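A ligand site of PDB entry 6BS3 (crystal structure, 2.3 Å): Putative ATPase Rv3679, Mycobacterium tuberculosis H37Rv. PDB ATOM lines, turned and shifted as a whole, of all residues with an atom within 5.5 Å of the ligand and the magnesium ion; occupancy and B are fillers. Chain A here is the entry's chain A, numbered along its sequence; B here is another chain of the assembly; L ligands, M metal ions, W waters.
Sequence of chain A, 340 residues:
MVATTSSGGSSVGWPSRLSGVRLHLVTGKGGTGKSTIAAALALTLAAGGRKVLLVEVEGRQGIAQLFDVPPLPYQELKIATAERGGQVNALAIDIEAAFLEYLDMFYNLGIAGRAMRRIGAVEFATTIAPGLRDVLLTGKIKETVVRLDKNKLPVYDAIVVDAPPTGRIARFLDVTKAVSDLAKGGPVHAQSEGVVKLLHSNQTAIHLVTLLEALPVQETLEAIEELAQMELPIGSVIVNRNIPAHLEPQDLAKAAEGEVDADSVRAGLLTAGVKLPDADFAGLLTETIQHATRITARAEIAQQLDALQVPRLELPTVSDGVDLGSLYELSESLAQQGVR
N of Thr 36 is in hydrogen-bond range of O5 of the ligand. The backbone NH (N) of Ser 35 lies close to an oxygen (O1) of the ligand, at 3.1 Å. The side-chain amino group (NZ) of Lys 34 lies within salt-bridge range of an oxygen (O3) of the ligand, at 2.8 Å. N4 of the ligand is in hydrogen-bond range of N of Val 318 (3.0 Å). A nitrogen (N2) of the ligand lies within hydrogen-bond range of the side-chain amide nitrogen of Asn 240. The backbone NH (N) of Lys 34 is in hydrogen-bond range of an oxygen (O3) of the ligand. O of Pro 316 lies within hydrogen-bond range of N3 of the ligand. O3 of the ligand lies within hydrogen-bond range of N of Gly 33 (3.1 Å). The side-chain carboxylate (OD2) of Asp 258 of chain B sits at hydrogen-bond distance from an oxygen (O9) of the ligand (2.7 Å). An oxygen (O5) of the ligand sits at hydrogen-bond distance from the side-chain hydroxyl of Thr 36. The backbone NH (N) of Thr 32 sits at hydrogen-bond distance from an oxygen (O3) of the ligand, at 3.4 Å. The backbone NH of Gly 31 is in hydrogen-bond range of an oxygen (O2) of the ligand (2.9 Å).
Arg 60 touches the magnesium ion (NH1 to MG, 3.95 Å). Two residues have an atom within 4 Å of the magnesium ion: Ser 35 and Arg 60. Along chain A the residues within 4 Å of the magnesium ion span positions 35 to 60. The nearest printed residue that does not touch the magnesium ion is Asp 162 (4.3 Å).
The backbone carbonyl oxygen of Gly 28 lies within hydrogen-bond range of the side-chain amino group of Lys 34, at 3.0 Å. The side-chain carboxylate (OD2) of Asp 162 sits close to the side-chain hydroxyl (OG) of Ser 35, 2.7 Å away. O of Arg 241 sits close to OG1 of Thr 317 (3.3 Å). The side-chain amide nitrogen (ND2) of Asn 240 lies within hydrogen-bond range of the backbone carbonyl oxygen (O) of Thr 32, at 2.8 Å. O of Lys 29 lies within hydrogen-bond range of NZ of Lys 34, 3.1 Å away. The backbone carbonyl oxygen of Leu 315 is in hydrogen-bond range of the backbone NH of Arg 241 (3.4 Å). The side-chain hydroxyl (OG1) of Thr 32 lies within hydrogen-bond range of the backbone carbonyl oxygen (O) of Lys 29 (2.7 Å).
Water W4 bridges O2 of the ligand and NH2 of Arg 60.
Lys 29 touches the ligand (O to O3, 3.7 Å). C of Gly 30 touches O2 of the ligand (3.98 Å). Arg 241 touches the ligand (CG to C8, 3.6 Å). Thr 317 touches the ligand. CG2 of Val 322 touches C10 of the ligand (3.5 Å). Leu 330 touches the ligand (CD2 to N3, 3.9 Å). Hydrophobic or aromatic side chains that line the ligand: Val 318, Val 322 and Leu 330. Within 4 Å of the ligand: Lys 29, Gly 30, Gly 31, Thr 32, Gly 33, Lys 34, Ser 35, Thr 36, Asn 240, Arg 241, Pro 316, Thr 317, Val 318, Val 322, Leu 330 and Asp 258 of chain B.
The magnesium ion is bound by water W5 (2.0 Å), water W1 (2.1 Å), water W3 (2.1 Å), O1 of the ligand (2.2 Å), OG of Ser 35 (2.3 Å) and water W4 (2.4 Å).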
ATOM      1  N   GLY A  28       9.139  19.512  31.969  1.00  0.00           N
ATOM      2  CA  GLY A  28       8.243  20.648  31.796  1.00  0.00           C
ATOM      3  C   GLY A  28       7.157  20.636  32.857  1.00  0.00           C
ATOM      4  O   GLY A  28       6.943  19.609  33.506  1.00  0.00           O
ATOM      5  N   LYS A  29       6.487  21.765  33.073  1.00  0.00           N
ATOM      6  CA  LYS A  29       5.410  21.838  34.064  1.00  0.00           C
ATOM      7  C   LYS A  29       4.242  20.907  33.650  1.00  0.00           C
ATOM      8  O   LYS A  29       4.107  20.599  32.468  1.00  0.00           O
ATOM      9  CB  LYS A  29       4.960  23.308  34.189  1.00  0.00           C
ATOM     10  CG  LYS A  29       3.904  23.553  35.245  1.00  0.00           C
ATOM     11  CD  LYS A  29       3.794  25.029  35.655  1.00  0.00           C
ATOM     12  CE  LYS A  29       2.494  25.305  36.366  1.00  0.00           C
ATOM     13  NZ  LYS A  29       2.378  24.557  37.626  1.00  0.00           N
ATOM     14  N   GLY A  30       3.439  20.434  34.611  1.00  0.00           N
ATOM     15  CA  GLY A  30       2.283  19.598  34.310  1.00  0.00           C
ATOM     16  C   GLY A  30       1.353  20.310  33.332  1.00  0.00           C
ATOM     17  O   GLY A  30       1.175  21.539  33.421  1.00  0.00           O
ATOM     18  N   GLY A  31       0.827  19.559  32.358  1.00  0.00           N
ATOM     19  CA  GLY A  31      -0.081  20.063  31.330  1.00  0.00           C
ATOM     20  C   GLY A  31       0.566  20.829  30.191  1.00  0.00           C
ATOM     21  O   GLY A  31      -0.158  21.384  29.358  1.00  0.00           O
ATOM     22  N   THR A  32       1.909  20.891  30.112  1.00  0.00           N
ATOM     23  CA  THR A  32       2.570  21.633  29.015  1.00  0.00           C
ATOM     24  C   THR A  32       2.758  20.783  27.749  1.00  0.00           C
ATOM     25  O   THR A  32       2.907  21.344  26.666  1.00  0.00           O
ATOM     26  CB  THR A  32       3.868  22.290  29.459  1.00  0.00           C
ATOM     27  OG1 THR A  32       4.755  21.291  29.978  1.00  0.00           O
ATOM     28  CG2 THR A  32       3.634  23.400  30.499  1.00  0.00           C
ATOM     29  N   GLY A  33       2.739  19.461  27.880  1.00  0.00           N
ATOM     30  CA  GLY A  33       2.873  18.564  26.738  1.00  0.00           C
ATOM     31  C   GLY A  33       4.029  17.591  26.739  1.00  0.00           C
ATOM     32  O   GLY A  33       4.385  17.103  25.661  1.00  0.00           O
ATOM     33  N   LYS A  34       4.624  17.284  27.906  1.00  0.00           N
ATOM     34  CA  LYS A  34       5.749  16.334  28.038  1.00  0.00           C
ATOM     35  C   LYS A  34       5.471  14.991  27.360  1.00  0.00           C
ATOM     36  O   LYS A  34       6.303  14.536  26.570  1.00  0.00           O
ATOM     37  CB  LYS A  34       6.079  16.051  29.509  1.00  0.00           C
ATOM     38  CG  LYS A  34       6.732  17.181  30.284  1.00  0.00           C
ATOM     39  CD  LYS A  34       7.028  16.731  31.742  1.00  0.00           C
ATOM     40  CE  LYS A  34       5.774  16.443  32.552  1.00  0.00           C
ATOM     41  NZ  LYS A  34       4.850  17.618  32.601  1.00  0.00           N
ATOM     42  N   SER A  35       4.339  14.346  27.696  1.00  0.00           N
ATOM     43  CA  SER A  35       3.946  13.047  27.147  1.00  0.00           C
ATOM     44  C   SER A  35       3.771  13.059  25.652  1.00  0.00           C
ATOM     45  O   SER A  35       4.296  12.183  24.977  1.00  0.00           O
ATOM     46  CB  SER A  35       2.694  12.501  27.830  1.00  0.00           C
ATOM     47  OG  SER A  35       2.887  12.287  29.215  1.00  0.00           O
ATOM     48  N   THR A  36       3.014  14.033  25.130  1.00  0.00           N
ATOM     49  CA  THR A  36       2.760  14.236  23.693  1.00  0.00           C
ATOM     50  C   THR A  36       4.078  14.449  22.915  1.00  0.00           C
ATOM     51  O   THR A  36       4.287  13.822  21.886  1.00  0.00           O
ATOM     52  CB  THR A  36       1.825  15.448  23.489  1.00  0.00           C
ATOM     53  OG1 THR A  36       0.659  15.279  24.271  1.00  0.00           O
ATOM     54  CG2 THR A  36       1.422  15.630  22.048  1.00  0.00           C
ATOM     55  N   ILE A  37       4.917  15.383  23.399  1.00  0.00           N
ATOM     56  CA  ILE A  37       6.186  15.792  22.774  1.00  0.00           C
ATOM     57  C   ILE A  37       7.270  14.696  22.899  1.00  0.00           C
ATOM     58  O   ILE A  37       8.059  14.541  21.974  1.00  0.00           O
ATOM     59  CB  ILE A  37       6.637  17.170  23.328  1.00  0.00           C
ATOM     60  CG1 ILE A  37       5.563  18.242  22.989  1.00  0.00           C
ATOM     61  CG2 ILE A  37       8.036  17.577  22.826  1.00  0.00           C
ATOM     62  CD1 ILE A  37       5.848  19.607  23.460  1.00  0.00           C
ATOM     63  N   ARG A  60       1.709   6.258  35.786  1.00  0.00           N
ATOM     64  CA  ARG A  60       0.499   6.923  35.330  1.00  0.00           C
ATOM     65  C   ARG A  60      -0.115   6.335  34.046  1.00  0.00           C
ATOM     66  O   ARG A  60      -1.221   6.750  33.667  1.00  0.00           O
ATOM     67  CB  ARG A  60       0.773   8.423  35.178  1.00  0.00           C
ATOM     68  CG  ARG A  60       0.997   9.106  36.537  1.00  0.00           C
ATOM     69  CD  ARG A  60       1.555  10.497  36.407  1.00  0.00           C
ATOM     70  NE  ARG A  60       0.564  11.426  35.849  1.00  0.00           N
ATOM     71  CZ  ARG A  60       0.859  12.549  35.202  1.00  0.00           C
ATOM     72  NH1 ARG A  60       2.131  12.907  35.018  1.00  0.00           N
ATOM     73  NH2 ARG A  60      -0.105  13.316  34.721  1.00  0.00           N
ATOM     74  N   ASP A 162       9.733  10.322  29.072  1.00  0.00           N
ATOM     75  CA  ASP A 162       8.630  11.207  29.428  1.00  0.00           C
ATOM     76  C   ASP A 162       8.907  11.292  30.954  1.00  0.00           C
ATOM     77  O   ASP A 162       8.576  10.386  31.719  1.00  0.00           O
ATOM     78  CB  ASP A 162       7.296  10.533  29.076  1.00  0.00           C
ATOM     79  CG  ASP A 162       6.009  11.181  29.545  1.00  0.00           C
ATOM     80  OD1 ASP A 162       6.064  12.268  30.157  1.00  0.00           O
ATOM     81  OD2 ASP A 162       4.943  10.587  29.329  1.00  0.00           O
ATOM     82  N   ASN A 240       5.619  24.752  23.199  1.00  0.00           N
ATOM     83  CA  ASN A 240       4.438  24.072  22.680  1.00  0.00           C
ATOM     84  C   ASN A 240       3.247  25.035  22.502  1.00  0.00           C
ATOM     85  O   ASN A 240       3.227  26.134  23.073  1.00  0.00           O
ATOM     86  CB  ASN A 240       4.050  22.925  23.640  1.00  0.00           C
ATOM     87  CG  ASN A 240       3.166  21.858  23.052  1.00  0.00           C
ATOM     88  OD1 ASN A 240       3.098  21.670  21.829  1.00  0.00           O
ATOM     89  ND2 ASN A 240       2.466  21.134  23.911  1.00  0.00           N
ATOM     90  N   ARG A 241       2.263  24.584  21.692  1.00  0.00           N
ATOM     91  CA  ARG A 241       0.965  25.223  21.396  1.00  0.00           C
ATOM     92  C   ARG A 241       1.078  26.694  21.009  1.00  0.00           C
ATOM     93  O   ARG A 241       0.407  27.550  21.596  1.00  0.00           O
ATOM     94  CB  ARG A 241      -0.069  25.033  22.520  1.00  0.00           C
ATOM     95  CG  ARG A 241      -0.233  23.597  22.950  1.00  0.00           C
ATOM     96  CD  ARG A 241      -1.575  23.326  23.593  1.00  0.00           C
ATOM     97  NE  ARG A 241      -1.839  24.208  24.725  1.00  0.00           N
ATOM     98  CZ  ARG A 241      -2.967  24.203  25.420  1.00  0.00           C
ATOM     99  NH1 ARG A 241      -3.935  23.335  25.131  1.00  0.00           N
ATOM    100  NH2 ARG A 241      -3.137  25.047  26.426  1.00  0.00           N
ATOM    101  N   LEU A 315       6.383  24.252  18.485  1.00  0.00           N
ATOM    102  CA  LEU A 315       5.367  23.377  17.947  1.00  0.00           C
ATOM    103  C   LEU A 315       4.035  24.122  17.856  1.00  0.00           C
ATOM    104  O   LEU A 315       3.766  25.021  18.673  1.00  0.00           O
ATOM    105  CB  LEU A 315       5.224  22.105  18.819  1.00  0.00           C
ATOM    106  CG  LEU A 315       6.453  21.182  18.851  1.00  0.00           C
ATOM    107  CD1 LEU A 315       6.273  20.095  19.861  1.00  0.00           C
ATOM    108  CD2 LEU A 315       6.734  20.578  17.479  1.00  0.00           C
ATOM    109  N   PRO A 316       3.199  23.815  16.835  1.00  0.00           N
ATOM    110  CA  PRO A 316       1.910  24.494  16.726  1.00  0.00           C
ATOM    111  C   PRO A 316       0.862  23.855  17.669  1.00  0.00           C
ATOM    112  O   PRO A 316       1.143  22.892  18.397  1.00  0.00           O
ATOM    113  CB  PRO A 316       1.527  24.260  15.257  1.00  0.00           C
ATOM    114  CG  PRO A 316       2.084  22.874  14.960  1.00  0.00           C
ATOM    115  CD  PRO A 316       3.369  22.792  15.761  1.00  0.00           C
ATOM    116  N   THR A 317      -0.356  24.422  17.643  1.00  0.00           N
ATOM    117  CA  THR A 317      -1.506  23.924  18.364  1.00  0.00           C
ATOM    118  C   THR A 317      -2.252  23.023  17.369  1.00  0.00           C
ATOM    119  O   THR A 317      -2.560  23.462  16.253  1.00  0.00           O
ATOM    120  CB  THR A 317      -2.446  25.097  18.765  1.00  0.00           C
ATOM    121  OG1 THR A 317      -1.782  25.962  19.678  1.00  0.00           O
ATOM    122  CG2 THR A 317      -3.773  24.619  19.364  1.00  0.00           C
ATOM    123  N   VAL A 318      -2.550  21.793  17.792  1.00  0.00           N
ATOM    124  CA  VAL A 318      -3.366  20.831  17.043  1.00  0.00           C
ATOM    125  C   VAL A 318      -4.826  21.257  17.355  1.00  0.00           C
ATOM    126  O   VAL A 318      -5.226  21.271  18.514  1.00  0.00           O
ATOM    127  CB  VAL A 318      -3.029  19.375  17.448  1.00  0.00           C
ATOM    128  CG1 VAL A 318      -4.056  18.398  16.887  1.00  0.00           C
ATOM    129  CG2 VAL A 318      -1.621  18.984  17.001  1.00  0.00           C
ATOM    130  N   ASP A 320      -7.956  20.323  17.061  1.00  0.00           N
ATOM    131  CA  ASP A 320      -8.835  19.398  17.824  1.00  0.00           C
ATOM    132  C   ASP A 320      -7.975  18.603  18.816  1.00  0.00           C
ATOM    133  O   ASP A 320      -6.850  19.037  19.103  1.00  0.00           O
ATOM    134  CB  ASP A 320      -9.637  18.479  16.891  1.00  0.00           C
ATOM    135  CG  ASP A 320     -10.612  19.224  16.005  1.00  0.00           C
ATOM    136  OD1 ASP A 320     -10.303  19.413  14.811  1.00  0.00           O
ATOM    137  OD2 ASP A 320     -11.677  19.630  16.510  1.00  0.00           O
ATOM    138  N   VAL A 322      -5.563  15.627  20.487  1.00  0.00           N
ATOM    139  CA  VAL A 322      -4.317  15.037  20.002  1.00  0.00           C
ATOM    140  C   VAL A 322      -4.654  13.555  19.755  1.00  0.00           C
ATOM    141  O   VAL A 322      -5.019  12.847  20.679  1.00  0.00           O
ATOM    142  CB  VAL A 322      -3.112  15.247  20.972  1.00  0.00           C
ATOM    143  CG1 VAL A 322      -1.940  14.324  20.616  1.00  0.00           C
ATOM    144  CG2 VAL A 322      -2.654  16.699  20.973  1.00  0.00           C
ATOM    145  N   LEU A 330       3.215  16.569  14.745  1.00  0.00           N
ATOM    146  CA  LEU A 330       4.180  17.185  15.668  1.00  0.00           C
ATOM    147  C   LEU A 330       5.600  16.654  15.417  1.00  0.00           C
ATOM    148  O   LEU A 330       6.543  17.434  15.483  1.00  0.00           O
ATOM    149  CB  LEU A 330       3.766  17.018  17.134  1.00  0.00           C
ATOM    150  CG  LEU A 330       2.459  17.701  17.570  1.00  0.00           C
ATOM    151  CD1 LEU A 330       2.100  17.292  18.985  1.00  0.00           C
ATOM    152  CD2 LEU A 330       2.553  19.239  17.488  1.00  0.00           C
ATOM    153  N   ARG B 159      -4.890  16.674  37.654  1.00  0.00           N
ATOM    154  CA  ARG B 159      -5.436  16.251  36.360  1.00  0.00           C
ATOM    155  C   ARG B 159      -6.787  15.574  36.645  1.00  0.00           C
ATOM    156  O   ARG B 159      -7.656  15.550  35.774  1.00  0.00           O
ATOM    157  CB  ARG B 159      -4.503  15.250  35.660  1.00  0.00           C
ATOM    158  CG  ARG B 159      -3.478  15.913  34.734  1.00  0.00           C
ATOM    159  CD  ARG B 159      -3.319  15.157  33.414  1.00  0.00           C
ATOM    160  NE  ARG B 159      -2.841  13.777  33.608  1.00  0.00           N
ATOM    161  CZ  ARG B 159      -3.502  12.680  33.228  1.00  0.00           C
ATOM    162  NH1 ARG B 159      -4.674  12.788  32.609  1.00  0.00           N
ATOM    163  NH2 ARG B 159      -2.991  11.485  33.448  1.00  0.00           N
ATOM    164  N   ASP B 258     -10.686  17.776  28.146  1.00  0.00           N
ATOM    165  CA  ASP B 258     -10.203  17.115  29.368  1.00  0.00           C
ATOM    166  C   ASP B 258     -10.815  17.714  30.628  1.00  0.00           C
ATOM    167  O   ASP B 258     -11.340  16.956  31.464  1.00  0.00           O
ATOM    168  CB  ASP B 258      -8.666  17.151  29.437  1.00  0.00           C
ATOM    169  CG  ASP B 258      -7.971  16.215  28.466  1.00  0.00           C
ATOM    170  OD1 ASP B 258      -8.654  15.377  27.843  1.00  0.00           O
ATOM    171  OD2 ASP B 258      -6.729  16.314  28.340  1.00  0.00           O
HETATM  172  P1  LIG L   1       2.035  16.719  30.265  1.00  0.00           P
HETATM  173  O1  LIG L   1       2.517  15.256  30.099  1.00  0.00           O
HETATM  174  O2  LIG L   1       1.067  16.804  31.471  1.00  0.00           O
HETATM  175  O3  LIG L   1       3.160  17.723  30.375  1.00  0.00           O
HETATM  176  P2  LIG L   1       0.300  16.270  27.914  1.00  0.00           P
HETATM  177  O4  LIG L   1      -0.578  15.203  28.605  1.00  0.00           O
HETATM  178  O5  LIG L   1       1.170  15.669  26.876  1.00  0.00           O
HETATM  179  O6  LIG L   1       1.147  17.055  29.001  1.00  0.00           O
HETATM  180  O7  LIG L   1      -0.566  17.491  27.400  1.00  0.00           O
HETATM  181  C1  LIG L   1      -1.574  18.219  28.148  1.00  0.00           C
HETATM  182  C2  LIG L   1      -2.797  18.346  27.272  1.00  0.00           C
HETATM  183  O8  LIG L   1      -2.491  19.172  26.140  1.00  0.00           O
HETATM  184  C3  LIG L   1      -3.357  17.046  26.690  1.00  0.00           C
HETATM  185  O9  LIG L   1      -4.776  17.097  26.662  1.00  0.00           O
HETATM  186  C4  LIG L   1      -2.749  17.004  25.286  1.00  0.00           C
HETATM  187  O10 LIG L   1      -3.481  16.208  24.354  1.00  0.00           O
HETATM  188  C5  LIG L   1      -2.736  18.488  24.929  1.00  0.00           C
HETATM  189  N1  LIG L   1      -1.716  18.883  23.957  1.00  0.00           N
HETATM  190  C6  LIG L   1      -0.356  18.701  24.040  1.00  0.00           C
HETATM  191  N2  LIG L   1       0.315  19.238  23.053  1.00  0.00           N
HETATM  192  C7  LIG L   1      -0.664  19.807  22.252  1.00  0.00           C
HETATM  193  C8  LIG L   1      -0.594  20.562  21.066  1.00  0.00           C
HETATM  194  N3  LIG L   1       0.539  20.835  20.418  1.00  0.00           N
HETATM  195  N4  LIG L   1      -1.753  21.025  20.549  1.00  0.00           N
HETATM  196  C9  LIG L   1      -2.906  20.754  21.184  1.00  0.00           C
HETATM  197  N5  LIG L   1      -3.082  20.037  22.299  1.00  0.00           N
HETATM  198  C10 LIG L   1      -1.921  19.592  22.800  1.00  0.00           C
HETATM  199 MG    MG M   1       2.045  13.304  31.085  1.00  0.00          MG
HETATM  200  O   HOH W   1       0.257  13.093  30.024  1.00  0.00           O
HETATM  201  O   HOH W   2      -1.758  13.171  27.161  1.00  0.00           O
HETATM  202  O   HOH W   3       1.694  11.414  31.957  1.00  0.00           O
HETATM  203  O   HOH W   4       1.533  14.702  32.933  1.00  0.00           O
HETATM  204  O   HOH W   5       3.912  13.121  31.686  1.00  0.00           O
